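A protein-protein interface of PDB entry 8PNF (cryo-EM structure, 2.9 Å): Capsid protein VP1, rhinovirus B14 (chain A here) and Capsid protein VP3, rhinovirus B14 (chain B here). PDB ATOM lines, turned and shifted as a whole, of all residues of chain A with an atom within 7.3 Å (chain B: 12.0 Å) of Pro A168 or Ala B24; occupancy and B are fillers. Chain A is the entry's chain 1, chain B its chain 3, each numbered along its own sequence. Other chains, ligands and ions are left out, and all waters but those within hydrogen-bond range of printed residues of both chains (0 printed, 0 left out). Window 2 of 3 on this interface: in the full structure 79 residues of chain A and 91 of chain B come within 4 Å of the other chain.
Hydrophobic or aromatic side chains of chain B within 4 Å of the printed part of chain A: Ala B24, Leu B25 and Tyr B28. Along chain B the printed residues that touch a printed residue of chain A span positions 21 to 28. Of the 20 printed residues of chain A, 6 touch a printed residue of chain B. Hydrophobic or aromatic side chains of chain A that line the printed part of chain B: Tyr A146, Pro A168, Phe A180, Val A182 and Pro A183. Among the printed residues, no Asp or Glu carboxylate lies within 4 Å of a Lys or Arg side-chain nitrogen of the other chain.
Of chain B, only Ala B24 and Leu B25 come within 4 Å of Pro A168. Ala B24 touches just these residues of chain A: Pro A168, Phe A180 and Ser A181. No residue of chain B comes within 4 Å of Met A145. Ser A166 touches none of the printed residues of chain B. No residue of chain B comes within 4 Å of Ser A169. No residue of chain B comes within 4 Å of Val A170. Of chain B, only Ser B21, Pro B22 and Ala B24 come within 4 Å of Phe A180. Ser A181 touches just these residues of chain B: Ser B21 (3.3 Å), Pro B22 (2.7 Å), Ser B23 (3.2 Å) and Ala B24 (2.6 Å). Printed residues of chain A within 4 Å of Ser B21: Phe A180 (3.5 Å) and Ser A181 (3.3 Å). Of the printed residues of chain A, Ser B23 touches Ser A181 and Pro A183. Of the printed residues of chain A, Leu B25 touches Tyr A146 (3.9 Å), Pro A168 (3.7 Å), Val A182 (3.9 Å) and Pro A183 (3.9 Å). Of the printed residues of chain B, Pro A183 touches Ser B23 (3.9 Å), Leu B25 (3.9 Å) and Tyr B28 (3.6 Å). Pro B30 touches none of the printed residues of chain A. Glu B29 touches none of the printed residues of chain A. The nearest residue of chain B that does not touch Pro A168 is Pro B26 (6.1 Å). The nearest residue of chain A that does not touch Ala B24 is Val A182 (4.1 Å). The nearest printed residue of chain A that does not touch Ser B23 is Val A182 (5.1 Å).
The backbone NH of Tyr A122 sits at hydrogen-bond distance from the backbone carbonyl oxygen of Phe A180 (2.8 Å). The backbone carbonyl oxygen (O) of Pro A168 lies within hydrogen-bond range of the backbone NH (N) of Tyr A146, 2.7 Å away. The side-chain hydroxyl (OG) of Ser B23 lies within hydrogen-bond range of the backbone carbonyl oxygen (O) of Leu B25 (3.4 Å).
Among the printed residues, merely in contact across the chains: Tyr A146 with Leu B25 (3.9 Å), Pro A168 with Ala B24 (3.3 Å), Pro A168 with Leu B25 (3.7 Å), Phe A180 with Ser B21 (3.5 Å), Phe A180 with Pro B22 (3.4 Å), Phe A180 with Ala B24 (3.8 Å), Ser A181 with Ser B23 (3.2 Å), Val A182 with Leu B25 (3.9 Å), Pro A183 with Ser B23 (3.9 Å), Pro A183 with Leu B25 (3.9 Å) and Pro A183 with Tyr B28 (3.6 Å).
OG of Ser B21 is in hydrogen-bond range of N of Ser A181, at 3.3 Å. O of Pro B22 is in hydrogen-bond range of N of Ser A181. O of Ser A181 sits at hydrogen-bond distance from N of Ala B24.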
ATOM      1  N   TYR A 122     -33.238 -23.885 -14.616  1.00  0.00           N
ATOM      2  CA  TYR A 122     -34.192 -24.898 -14.197  1.00  0.00           C
ATOM      3  C   TYR A 122     -34.389 -24.843 -12.693  1.00  0.00           C
ATOM      4  O   TYR A 122     -33.436 -24.643 -11.937  1.00  0.00           O
ATOM      5  CB  TYR A 122     -33.736 -26.296 -14.607  1.00  0.00           C
ATOM      6  CG  TYR A 122     -33.716 -26.501 -16.093  1.00  0.00           C
ATOM      7  CD1 TYR A 122     -34.882 -26.785 -16.790  1.00  0.00           C
ATOM      8  CD2 TYR A 122     -32.530 -26.414 -16.805  1.00  0.00           C
ATOM      9  CE1 TYR A 122     -34.866 -26.971 -18.154  1.00  0.00           C
ATOM     10  CE2 TYR A 122     -32.506 -26.602 -18.166  1.00  0.00           C
ATOM     11  CZ  TYR A 122     -33.675 -26.879 -18.834  1.00  0.00           C
ATOM     12  OH  TYR A 122     -33.639 -27.060 -20.191  1.00  0.00           O
ATOM     13  N   GLN A 143     -32.852 -37.608  -6.796  1.00  0.00           N
ATOM     14  CA  GLN A 143     -31.796 -37.370  -7.766  1.00  0.00           C
ATOM     15  C   GLN A 143     -32.421 -37.014  -9.106  1.00  0.00           C
ATOM     16  O   GLN A 143     -33.267 -37.753  -9.618  1.00  0.00           O
ATOM     17  CB  GLN A 143     -30.896 -38.595  -7.923  1.00  0.00           C
ATOM     18  CG  GLN A 143     -30.021 -38.556  -9.163  1.00  0.00           C
ATOM     19  CD  GLN A 143     -28.926 -39.592  -9.143  1.00  0.00           C
ATOM     20  OE1 GLN A 143     -28.923 -40.493  -8.311  1.00  0.00           O
ATOM     21  NE2 GLN A 143     -27.984 -39.469 -10.064  1.00  0.00           N
ATOM     22  N   ALA A 144     -32.014 -35.876  -9.660  1.00  0.00           N
ATOM     23  CA  ALA A 144     -32.347 -35.485 -11.023  1.00  0.00           C
ATOM     24  C   ALA A 144     -31.034 -35.494 -11.794  1.00  0.00           C
ATOM     25  O   ALA A 144     -30.155 -34.671 -11.539  1.00  0.00           O
ATOM     26  CB  ALA A 144     -33.022 -34.125 -11.065  1.00  0.00           C
ATOM     27  N   MET A 145     -30.898 -36.427 -12.731  1.00  0.00           N
ATOM     28  CA  MET A 145     -29.674 -36.576 -13.503  1.00  0.00           C
ATOM     29  C   MET A 145     -29.900 -36.069 -14.921  1.00  0.00           C
ATOM     30  O   MET A 145     -30.782 -36.565 -15.623  1.00  0.00           O
ATOM     31  CB  MET A 145     -29.230 -38.035 -13.534  1.00  0.00           C
ATOM     32  CG  MET A 145     -28.014 -38.279 -14.387  1.00  0.00           C
ATOM     33  SD  MET A 145     -27.296 -39.911 -14.165  1.00  0.00           S
ATOM     34  CE  MET A 145     -28.624 -40.961 -14.722  1.00  0.00           C
ATOM     35  N   TYR A 146     -29.090 -35.107 -15.347  1.00  0.00           N
ATOM     36  CA  TYR A 146     -29.195 -34.578 -16.701  1.00  0.00           C
ATOM     37  C   TYR A 146     -28.485 -35.515 -17.668  1.00  0.00           C
ATOM     38  O   TYR A 146     -27.261 -35.652 -17.625  1.00  0.00           O
ATOM     39  CB  TYR A 146     -28.597 -33.176 -16.757  1.00  0.00           C
ATOM     40  CG  TYR A 146     -28.578 -32.538 -18.123  1.00  0.00           C
ATOM     41  CD1 TYR A 146     -29.734 -32.007 -18.682  1.00  0.00           C
ATOM     42  CD2 TYR A 146     -27.396 -32.434 -18.842  1.00  0.00           C
ATOM     43  CE1 TYR A 146     -29.714 -31.411 -19.925  1.00  0.00           C
ATOM     44  CE2 TYR A 146     -27.368 -31.840 -20.084  1.00  0.00           C
ATOM     45  CZ  TYR A 146     -28.529 -31.331 -20.620  1.00  0.00           C
ATOM     46  OH  TYR A 146     -28.500 -30.736 -21.856  1.00  0.00           O
ATOM     47  N   VAL A 147     -29.254 -36.164 -18.536  1.00  0.00           N
ATOM     48  CA  VAL A 147     -28.763 -37.221 -19.409  1.00  0.00           C
ATOM     49  C   VAL A 147     -28.659 -36.654 -20.823  1.00  0.00           C
ATOM     50  O   VAL A 147     -29.690 -36.402 -21.463  1.00  0.00           O
ATOM     51  CB  VAL A 147     -29.683 -38.449 -19.370  1.00  0.00           C
ATOM     52  CG1 VAL A 147     -29.116 -39.566 -20.218  1.00  0.00           C
ATOM     53  CG2 VAL A 147     -29.895 -38.908 -17.940  1.00  0.00           C
ATOM     54  N   PRO A 148     -27.457 -36.440 -21.350  1.00  0.00           N
ATOM     55  CA  PRO A 148     -27.313 -35.956 -22.731  1.00  0.00           C
ATOM     56  C   PRO A 148     -27.653 -37.048 -23.730  1.00  0.00           C
ATOM     57  O   PRO A 148     -27.741 -38.226 -23.356  1.00  0.00           O
ATOM     58  CB  PRO A 148     -25.826 -35.567 -22.808  1.00  0.00           C
ATOM     59  CG  PRO A 148     -25.372 -35.472 -21.389  1.00  0.00           C
ATOM     60  CD  PRO A 148     -26.164 -36.491 -20.655  1.00  0.00           C
ATOM     61  N   SER A 164     -23.119 -41.324 -12.286  1.00  0.00           N
ATOM     62  CA  SER A 164     -22.976 -40.051 -13.004  1.00  0.00           C
ATOM     63  C   SER A 164     -21.594 -39.423 -12.814  1.00  0.00           C
ATOM     64  O   SER A 164     -21.444 -38.348 -12.233  1.00  0.00           O
ATOM     65  CB  SER A 164     -24.075 -39.058 -12.609  1.00  0.00           C
ATOM     66  OG  SER A 164     -23.921 -38.590 -11.282  1.00  0.00           O
ATOM     67  N   ALA A 165     -20.578 -40.124 -13.311  1.00  0.00           N
ATOM     68  CA  ALA A 165     -19.233 -39.575 -13.286  1.00  0.00           C
ATOM     69  C   ALA A 165     -19.051 -38.447 -14.293  1.00  0.00           C
ATOM     70  O   ALA A 165     -18.191 -37.585 -14.088  1.00  0.00           O
ATOM     71  CB  ALA A 165     -18.208 -40.676 -13.543  1.00  0.00           C
ATOM     72  N   SER A 166     -19.843 -38.427 -15.363  1.00  0.00           N
ATOM     73  CA  SER A 166     -19.741 -37.376 -16.364  1.00  0.00           C
ATOM     74  C   SER A 166     -21.038 -36.584 -16.466  1.00  0.00           C
ATOM     75  O   SER A 166     -21.006 -35.368 -16.672  1.00  0.00           O
ATOM     76  CB  SER A 166     -19.376 -37.969 -17.723  1.00  0.00           C
ATOM     77  OG  SER A 166     -18.106 -38.585 -17.681  1.00  0.00           O
ATOM     78  N   ASN A 167     -22.174 -37.264 -16.339  1.00  0.00           N
ATOM     79  CA  ASN A 167     -23.470 -36.595 -16.416  1.00  0.00           C
ATOM     80  C   ASN A 167     -23.685 -35.717 -15.190  1.00  0.00           C
ATOM     81  O   ASN A 167     -23.420 -36.157 -14.068  1.00  0.00           O
ATOM     82  CB  ASN A 167     -24.605 -37.610 -16.514  1.00  0.00           C
ATOM     83  CG  ASN A 167     -24.526 -38.463 -17.756  1.00  0.00           C
ATOM     84  OD1 ASN A 167     -23.885 -38.096 -18.736  1.00  0.00           O
ATOM     85  ND2 ASN A 167     -25.204 -39.598 -17.731  1.00  0.00           N
ATOM     86  N   PRO A 168     -24.145 -34.477 -15.356  1.00  0.00           N
ATOM     87  CA  PRO A 168     -24.445 -33.642 -14.186  1.00  0.00           C
ATOM     88  C   PRO A 168     -25.742 -34.074 -13.515  1.00  0.00           C
ATOM     89  O   PRO A 168     -26.758 -34.293 -14.176  1.00  0.00           O
ATOM     90  CB  PRO A 168     -24.556 -32.233 -14.778  1.00  0.00           C
ATOM     91  CG  PRO A 168     -24.891 -32.448 -16.193  1.00  0.00           C
ATOM     92  CD  PRO A 168     -24.219 -33.711 -16.609  1.00  0.00           C
ATOM     93  N   SER A 169     -25.697 -34.193 -12.192  1.00  0.00           N
ATOM     94  CA  SER A 169     -26.857 -34.568 -11.401  1.00  0.00           C
ATOM     95  C   SER A 169     -26.946 -33.681 -10.167  1.00  0.00           C
ATOM     96  O   SER A 169     -25.961 -33.091  -9.727  1.00  0.00           O
ATOM     97  CB  SER A 169     -26.810 -36.043 -10.987  1.00  0.00           C
ATOM     98  OG  SER A 169     -25.607 -36.338 -10.309  1.00  0.00           O
ATOM     99  N   VAL A 170     -28.153 -33.579  -9.625  1.00  0.00           N
ATOM    100  CA  VAL A 170     -28.405 -32.797  -8.421  1.00  0.00           C
ATOM    101  C   VAL A 170     -29.169 -33.680  -7.441  1.00  0.00           C
ATOM    102  O   VAL A 170     -29.987 -34.508  -7.849  1.00  0.00           O
ATOM    103  CB  VAL A 170     -29.151 -31.477  -8.743  1.00  0.00           C
ATOM    104  CG1 VAL A 170     -30.501 -31.721  -9.401  1.00  0.00           C
ATOM    105  CG2 VAL A 170     -29.287 -30.582  -7.513  1.00  0.00           C
ATOM    106  N   PHE A 180     -30.631 -24.797 -10.879  1.00  0.00           N
ATOM    107  CA  PHE A 180     -29.365 -24.820 -11.594  1.00  0.00           C
ATOM    108  C   PHE A 180     -29.542 -24.168 -12.957  1.00  0.00           C
ATOM    109  O   PHE A 180     -30.647 -24.082 -13.496  1.00  0.00           O
ATOM    110  CB  PHE A 180     -28.810 -26.245 -11.736  1.00  0.00           C
ATOM    111  CG  PHE A 180     -29.765 -27.224 -12.363  1.00  0.00           C
ATOM    112  CD1 PHE A 180     -30.650 -27.948 -11.581  1.00  0.00           C
ATOM    113  CD2 PHE A 180     -29.749 -27.451 -13.729  1.00  0.00           C
ATOM    114  CE1 PHE A 180     -31.511 -28.851 -12.150  1.00  0.00           C
ATOM    115  CE2 PHE A 180     -30.615 -28.355 -14.301  1.00  0.00           C
ATOM    116  CZ  PHE A 180     -31.491 -29.058 -13.508  1.00  0.00           C
ATOM    117  N   SER A 181     -28.424 -23.726 -13.514  1.00  0.00           N
ATOM    118  CA  SER A 181     -28.376 -23.047 -14.798  1.00  0.00           C
ATOM    119  C   SER A 181     -27.800 -23.984 -15.847  1.00  0.00           C
ATOM    120  O   SER A 181     -26.837 -24.704 -15.588  1.00  0.00           O
ATOM    121  CB  SER A 181     -27.528 -21.781 -14.703  1.00  0.00           C
ATOM    122  OG  SER A 181     -27.464 -21.109 -15.942  1.00  0.00           O
ATOM    123  N   VAL A 182     -28.406 -23.992 -17.028  1.00  0.00           N
ATOM    124  CA  VAL A 182     -27.916 -24.753 -18.167  1.00  0.00           C
ATOM    125  C   VAL A 182     -27.719 -23.775 -19.317  1.00  0.00           C
ATOM    126  O   VAL A 182     -28.630 -23.004 -19.619  1.00  0.00           O
ATOM    127  CB  VAL A 182     -28.873 -25.887 -18.577  1.00  0.00           C
ATOM    128  CG1 VAL A 182     -28.390 -26.573 -19.831  1.00  0.00           C
ATOM    129  CG2 VAL A 182     -28.981 -26.898 -17.462  1.00  0.00           C
ATOM    130  N   PRO A 183     -26.552 -23.756 -19.970  1.00  0.00           N
ATOM    131  CA  PRO A 183     -26.335 -22.820 -21.082  1.00  0.00           C
ATOM    132  C   PRO A 183     -27.149 -23.129 -22.329  1.00  0.00           C
ATOM    133  O   PRO A 183     -27.957 -24.062 -22.350  1.00  0.00           O
ATOM    134  CB  PRO A 183     -24.833 -22.959 -21.362  1.00  0.00           C
ATOM    135  CG  PRO A 183     -24.445 -24.251 -20.746  1.00  0.00           C
ATOM    136  CD  PRO A 183     -25.305 -24.418 -19.561  1.00  0.00           C
ATOM    137  N   SER A 217     -32.084 -34.197 -21.785  1.00  0.00           N
ATOM    138  CA  SER A 217     -33.131 -34.892 -21.055  1.00  0.00           C
ATOM    139  C   SER A 217     -32.648 -35.096 -19.629  1.00  0.00           C
ATOM    140  O   SER A 217     -31.459 -35.301 -19.386  1.00  0.00           O
ATOM    141  CB  SER A 217     -33.484 -36.228 -21.711  1.00  0.00           C
ATOM    142  OG  SER A 217     -32.388 -37.116 -21.669  1.00  0.00           O
ATOM    143  N   MET A 218     -33.575 -35.018 -18.683  1.00  0.00           N
ATOM    144  CA  MET A 218     -33.238 -35.290 -17.295  1.00  0.00           C
ATOM    145  C   MET A 218     -34.086 -36.426 -16.742  1.00  0.00           C
ATOM    146  O   MET A 218     -35.284 -36.520 -17.016  1.00  0.00           O
ATOM    147  CB  MET A 218     -33.334 -34.028 -16.407  1.00  0.00           C
ATOM    148  CG  MET A 218     -34.693 -33.412 -16.261  1.00  0.00           C
ATOM    149  SD  MET A 218     -34.695 -31.900 -15.272  1.00  0.00           S
ATOM    150  CE  MET A 218     -33.940 -30.695 -16.344  1.00  0.00           C
ATOM    151  N   GLN B  20     -28.791 -15.438  -9.526  1.00  0.00           N
ATOM    152  CA  GLN B  20     -27.797 -16.308 -10.119  1.00  0.00           C
ATOM    153  C   GLN B  20     -27.952 -17.722  -9.571  1.00  0.00           C
ATOM    154  O   GLN B  20     -28.536 -17.943  -8.507  1.00  0.00           O
ATOM    155  CB  GLN B  20     -26.400 -15.779  -9.824  1.00  0.00           C
ATOM    156  CG  GLN B  20     -26.152 -14.398 -10.372  1.00  0.00           C
ATOM    157  CD  GLN B  20     -24.800 -13.866  -9.990  1.00  0.00           C
ATOM    158  OE1 GLN B  20     -24.038 -14.531  -9.303  1.00  0.00           O
ATOM    159  NE2 GLN B  20     -24.500 -12.652 -10.417  1.00  0.00           N
ATOM    160  N   SER B  21     -27.421 -18.691 -10.316  1.00  0.00           N
ATOM    161  CA  SER B  21     -27.556 -20.090  -9.943  1.00  0.00           C
ATOM    162  C   SER B  21     -26.387 -20.844 -10.544  1.00  0.00           C
ATOM    163  O   SER B  21     -25.833 -20.379 -11.547  1.00  0.00           O
ATOM    164  CB  SER B  21     -28.892 -20.661 -10.431  1.00  0.00           C
ATOM    165  OG  SER B  21     -28.851 -20.973 -11.805  1.00  0.00           O
ATOM    166  N   PRO B  22     -25.955 -21.964  -9.958  1.00  0.00           N
ATOM    167  CA  PRO B  22     -24.781 -22.665 -10.492  1.00  0.00           C
ATOM    168  C   PRO B  22     -25.040 -23.304 -11.846  1.00  0.00           C
ATOM    169  O   PRO B  22     -26.117 -23.836 -12.112  1.00  0.00           O
ATOM    170  CB  PRO B  22     -24.490 -23.723  -9.424  1.00  0.00           C
ATOM    171  CG  PRO B  22     -25.765 -23.885  -8.699  1.00  0.00           C
ATOM    172  CD  PRO B  22     -26.351 -22.519  -8.656  1.00  0.00           C
ATOM    173  N   SER B  23     -24.021 -23.261 -12.696  1.00  0.00           N
ATOM    174  CA  SER B  23     -24.123 -23.842 -14.022  1.00  0.00           C
ATOM    175  C   SER B  23     -23.914 -25.348 -13.950  1.00  0.00           C
ATOM    176  O   SER B  23     -22.903 -25.821 -13.424  1.00  0.00           O
ATOM    177  CB  SER B  23     -23.109 -23.208 -14.967  1.00  0.00           C
ATOM    178  OG  SER B  23     -23.327 -23.628 -16.299  1.00  0.00           O
ATOM    179  N   ALA B  24     -24.876 -26.101 -14.485  1.00  0.00           N
ATOM    180  CA  ALA B  24     -24.775 -27.554 -14.478  1.00  0.00           C
ATOM    181  C   ALA B  24     -23.777 -28.071 -15.504  1.00  0.00           C
ATOM    182  O   ALA B  24     -23.320 -29.210 -15.380  1.00  0.00           O
ATOM    183  CB  ALA B  24     -26.144 -28.182 -14.727  1.00  0.00           C
ATOM    184  N   LEU B  25     -23.416 -27.267 -16.502  1.00  0.00           N
ATOM    185  CA  LEU B  25     -22.433 -27.655 -17.511  1.00  0.00           C
ATOM    186  C   LEU B  25     -21.274 -26.675 -17.440  1.00  0.00           C
ATOM    187  O   LEU B  25     -21.265 -25.660 -18.150  1.00  0.00           O
ATOM    188  CB  LEU B  25     -23.038 -27.672 -18.912  1.00  0.00           C
ATOM    189  CG  LEU B  25     -24.392 -28.346 -19.122  1.00  0.00           C
ATOM    190  CD1 LEU B  25     -24.831 -28.120 -20.538  1.00  0.00           C
ATOM    191  CD2 LEU B  25     -24.335 -29.827 -18.814  1.00  0.00           C
ATOM    192  N   PRO B  26     -20.286 -26.925 -16.586  1.00  0.00           N
ATOM    193  CA  PRO B  26     -19.122 -26.043 -16.530  1.00  0.00           C
ATOM    194  C   PRO B  26     -18.245 -26.178 -17.764  1.00  0.00           C
ATOM    195  O   PRO B  26     -18.190 -27.229 -18.406  1.00  0.00           O
ATOM    196  CB  PRO B  26     -18.389 -26.509 -15.268  1.00  0.00           C
ATOM    197  CG  PRO B  26     -18.820 -27.895 -15.068  1.00  0.00           C
ATOM    198  CD  PRO B  26     -20.207 -28.009 -15.594  1.00  0.00           C
ATOM    199  N   ASN B  27     -17.607 -25.057 -18.111  1.00  0.00           N
ATOM    200  CA  ASN B  27     -16.686 -24.892 -19.239  1.00  0.00           C
ATOM    201  C   ASN B  27     -17.335 -25.142 -20.597  1.00  0.00           C
ATOM    202  O   ASN B  27     -16.632 -25.315 -21.594  1.00  0.00           O
ATOM    203  CB  ASN B  27     -15.438 -25.768 -19.084  1.00  0.00           C
ATOM    204  CG  ASN B  27     -14.632 -25.410 -17.867  1.00  0.00           C
ATOM    205  OD1 ASN B  27     -14.632 -26.133 -16.876  1.00  0.00           O
ATOM    206  ND2 ASN B  27     -13.937 -24.287 -17.931  1.00  0.00           N
ATOM    207  N   TYR B  28     -18.661 -25.131 -20.673  1.00  0.00           N
ATOM    208  CA  TYR B  28     -19.350 -25.366 -21.931  1.00  0.00           C
ATOM    209  C   TYR B  28     -19.273 -24.126 -22.812  1.00  0.00           C
ATOM    210  O   TYR B  28     -19.563 -23.012 -22.368  1.00  0.00           O
ATOM    211  CB  TYR B  28     -20.808 -25.750 -21.673  1.00  0.00           C
ATOM    212  CG  TYR B  28     -21.605 -26.084 -22.918  1.00  0.00           C
ATOM    213  CD1 TYR B  28     -21.602 -27.368 -23.441  1.00  0.00           C
ATOM    214  CD2 TYR B  28     -22.377 -25.119 -23.557  1.00  0.00           C
ATOM    215  CE1 TYR B  28     -22.324 -27.676 -24.572  1.00  0.00           C
ATOM    216  CE2 TYR B  28     -23.098 -25.419 -24.688  1.00  0.00           C
ATOM    217  CZ  TYR B  28     -23.072 -26.698 -25.185  1.00  0.00           C
ATOM    218  OH  TYR B  28     -23.799 -26.988 -26.311  1.00  0.00           O
ATOM    219  N   GLU B  29     -18.893 -24.332 -24.066  1.00  0.00           N
ATOM    220  CA  GLU B  29     -18.814 -23.260 -25.054  1.00  0.00           C
ATOM    221  C   GLU B  29     -19.948 -23.410 -26.052  1.00  0.00           C
ATOM    222  O   GLU B  29     -19.950 -24.375 -26.838  1.00  0.00           O
ATOM    223  CB  GLU B  29     -17.464 -23.284 -25.765  1.00  0.00           C
ATOM    224  CG  GLU B  29     -16.300 -23.451 -24.821  1.00  0.00           C
ATOM    225  CD  GLU B  29     -15.009 -23.745 -25.537  1.00  0.00           C
ATOM    226  OE1 GLU B  29     -14.505 -22.854 -26.248  1.00  0.00           O
ATOM    227  OE2 GLU B  29     -14.499 -24.874 -25.399  1.00  0.00           O
ATOM    228  N   PRO B  30     -20.930 -22.515 -26.058  1.00  0.00           N
ATOM    229  CA  PRO B  30     -22.073 -22.677 -26.960  1.00  0.00           C
ATOM    230  C   PRO B  30     -21.732 -22.287 -28.388  1.00  0.00           C
ATOM    231  O   PRO B  30     -20.652 -21.782 -28.693  1.00  0.00           O
ATOM    232  CB  PRO B  30     -23.133 -21.751 -26.358  1.00  0.00           C
ATOM    233  CG  PRO B  30     -22.370 -20.759 -25.590  1.00  0.00           C
ATOM    234  CD  PRO B  30     -21.150 -21.439 -25.079  1.00  0.00           C
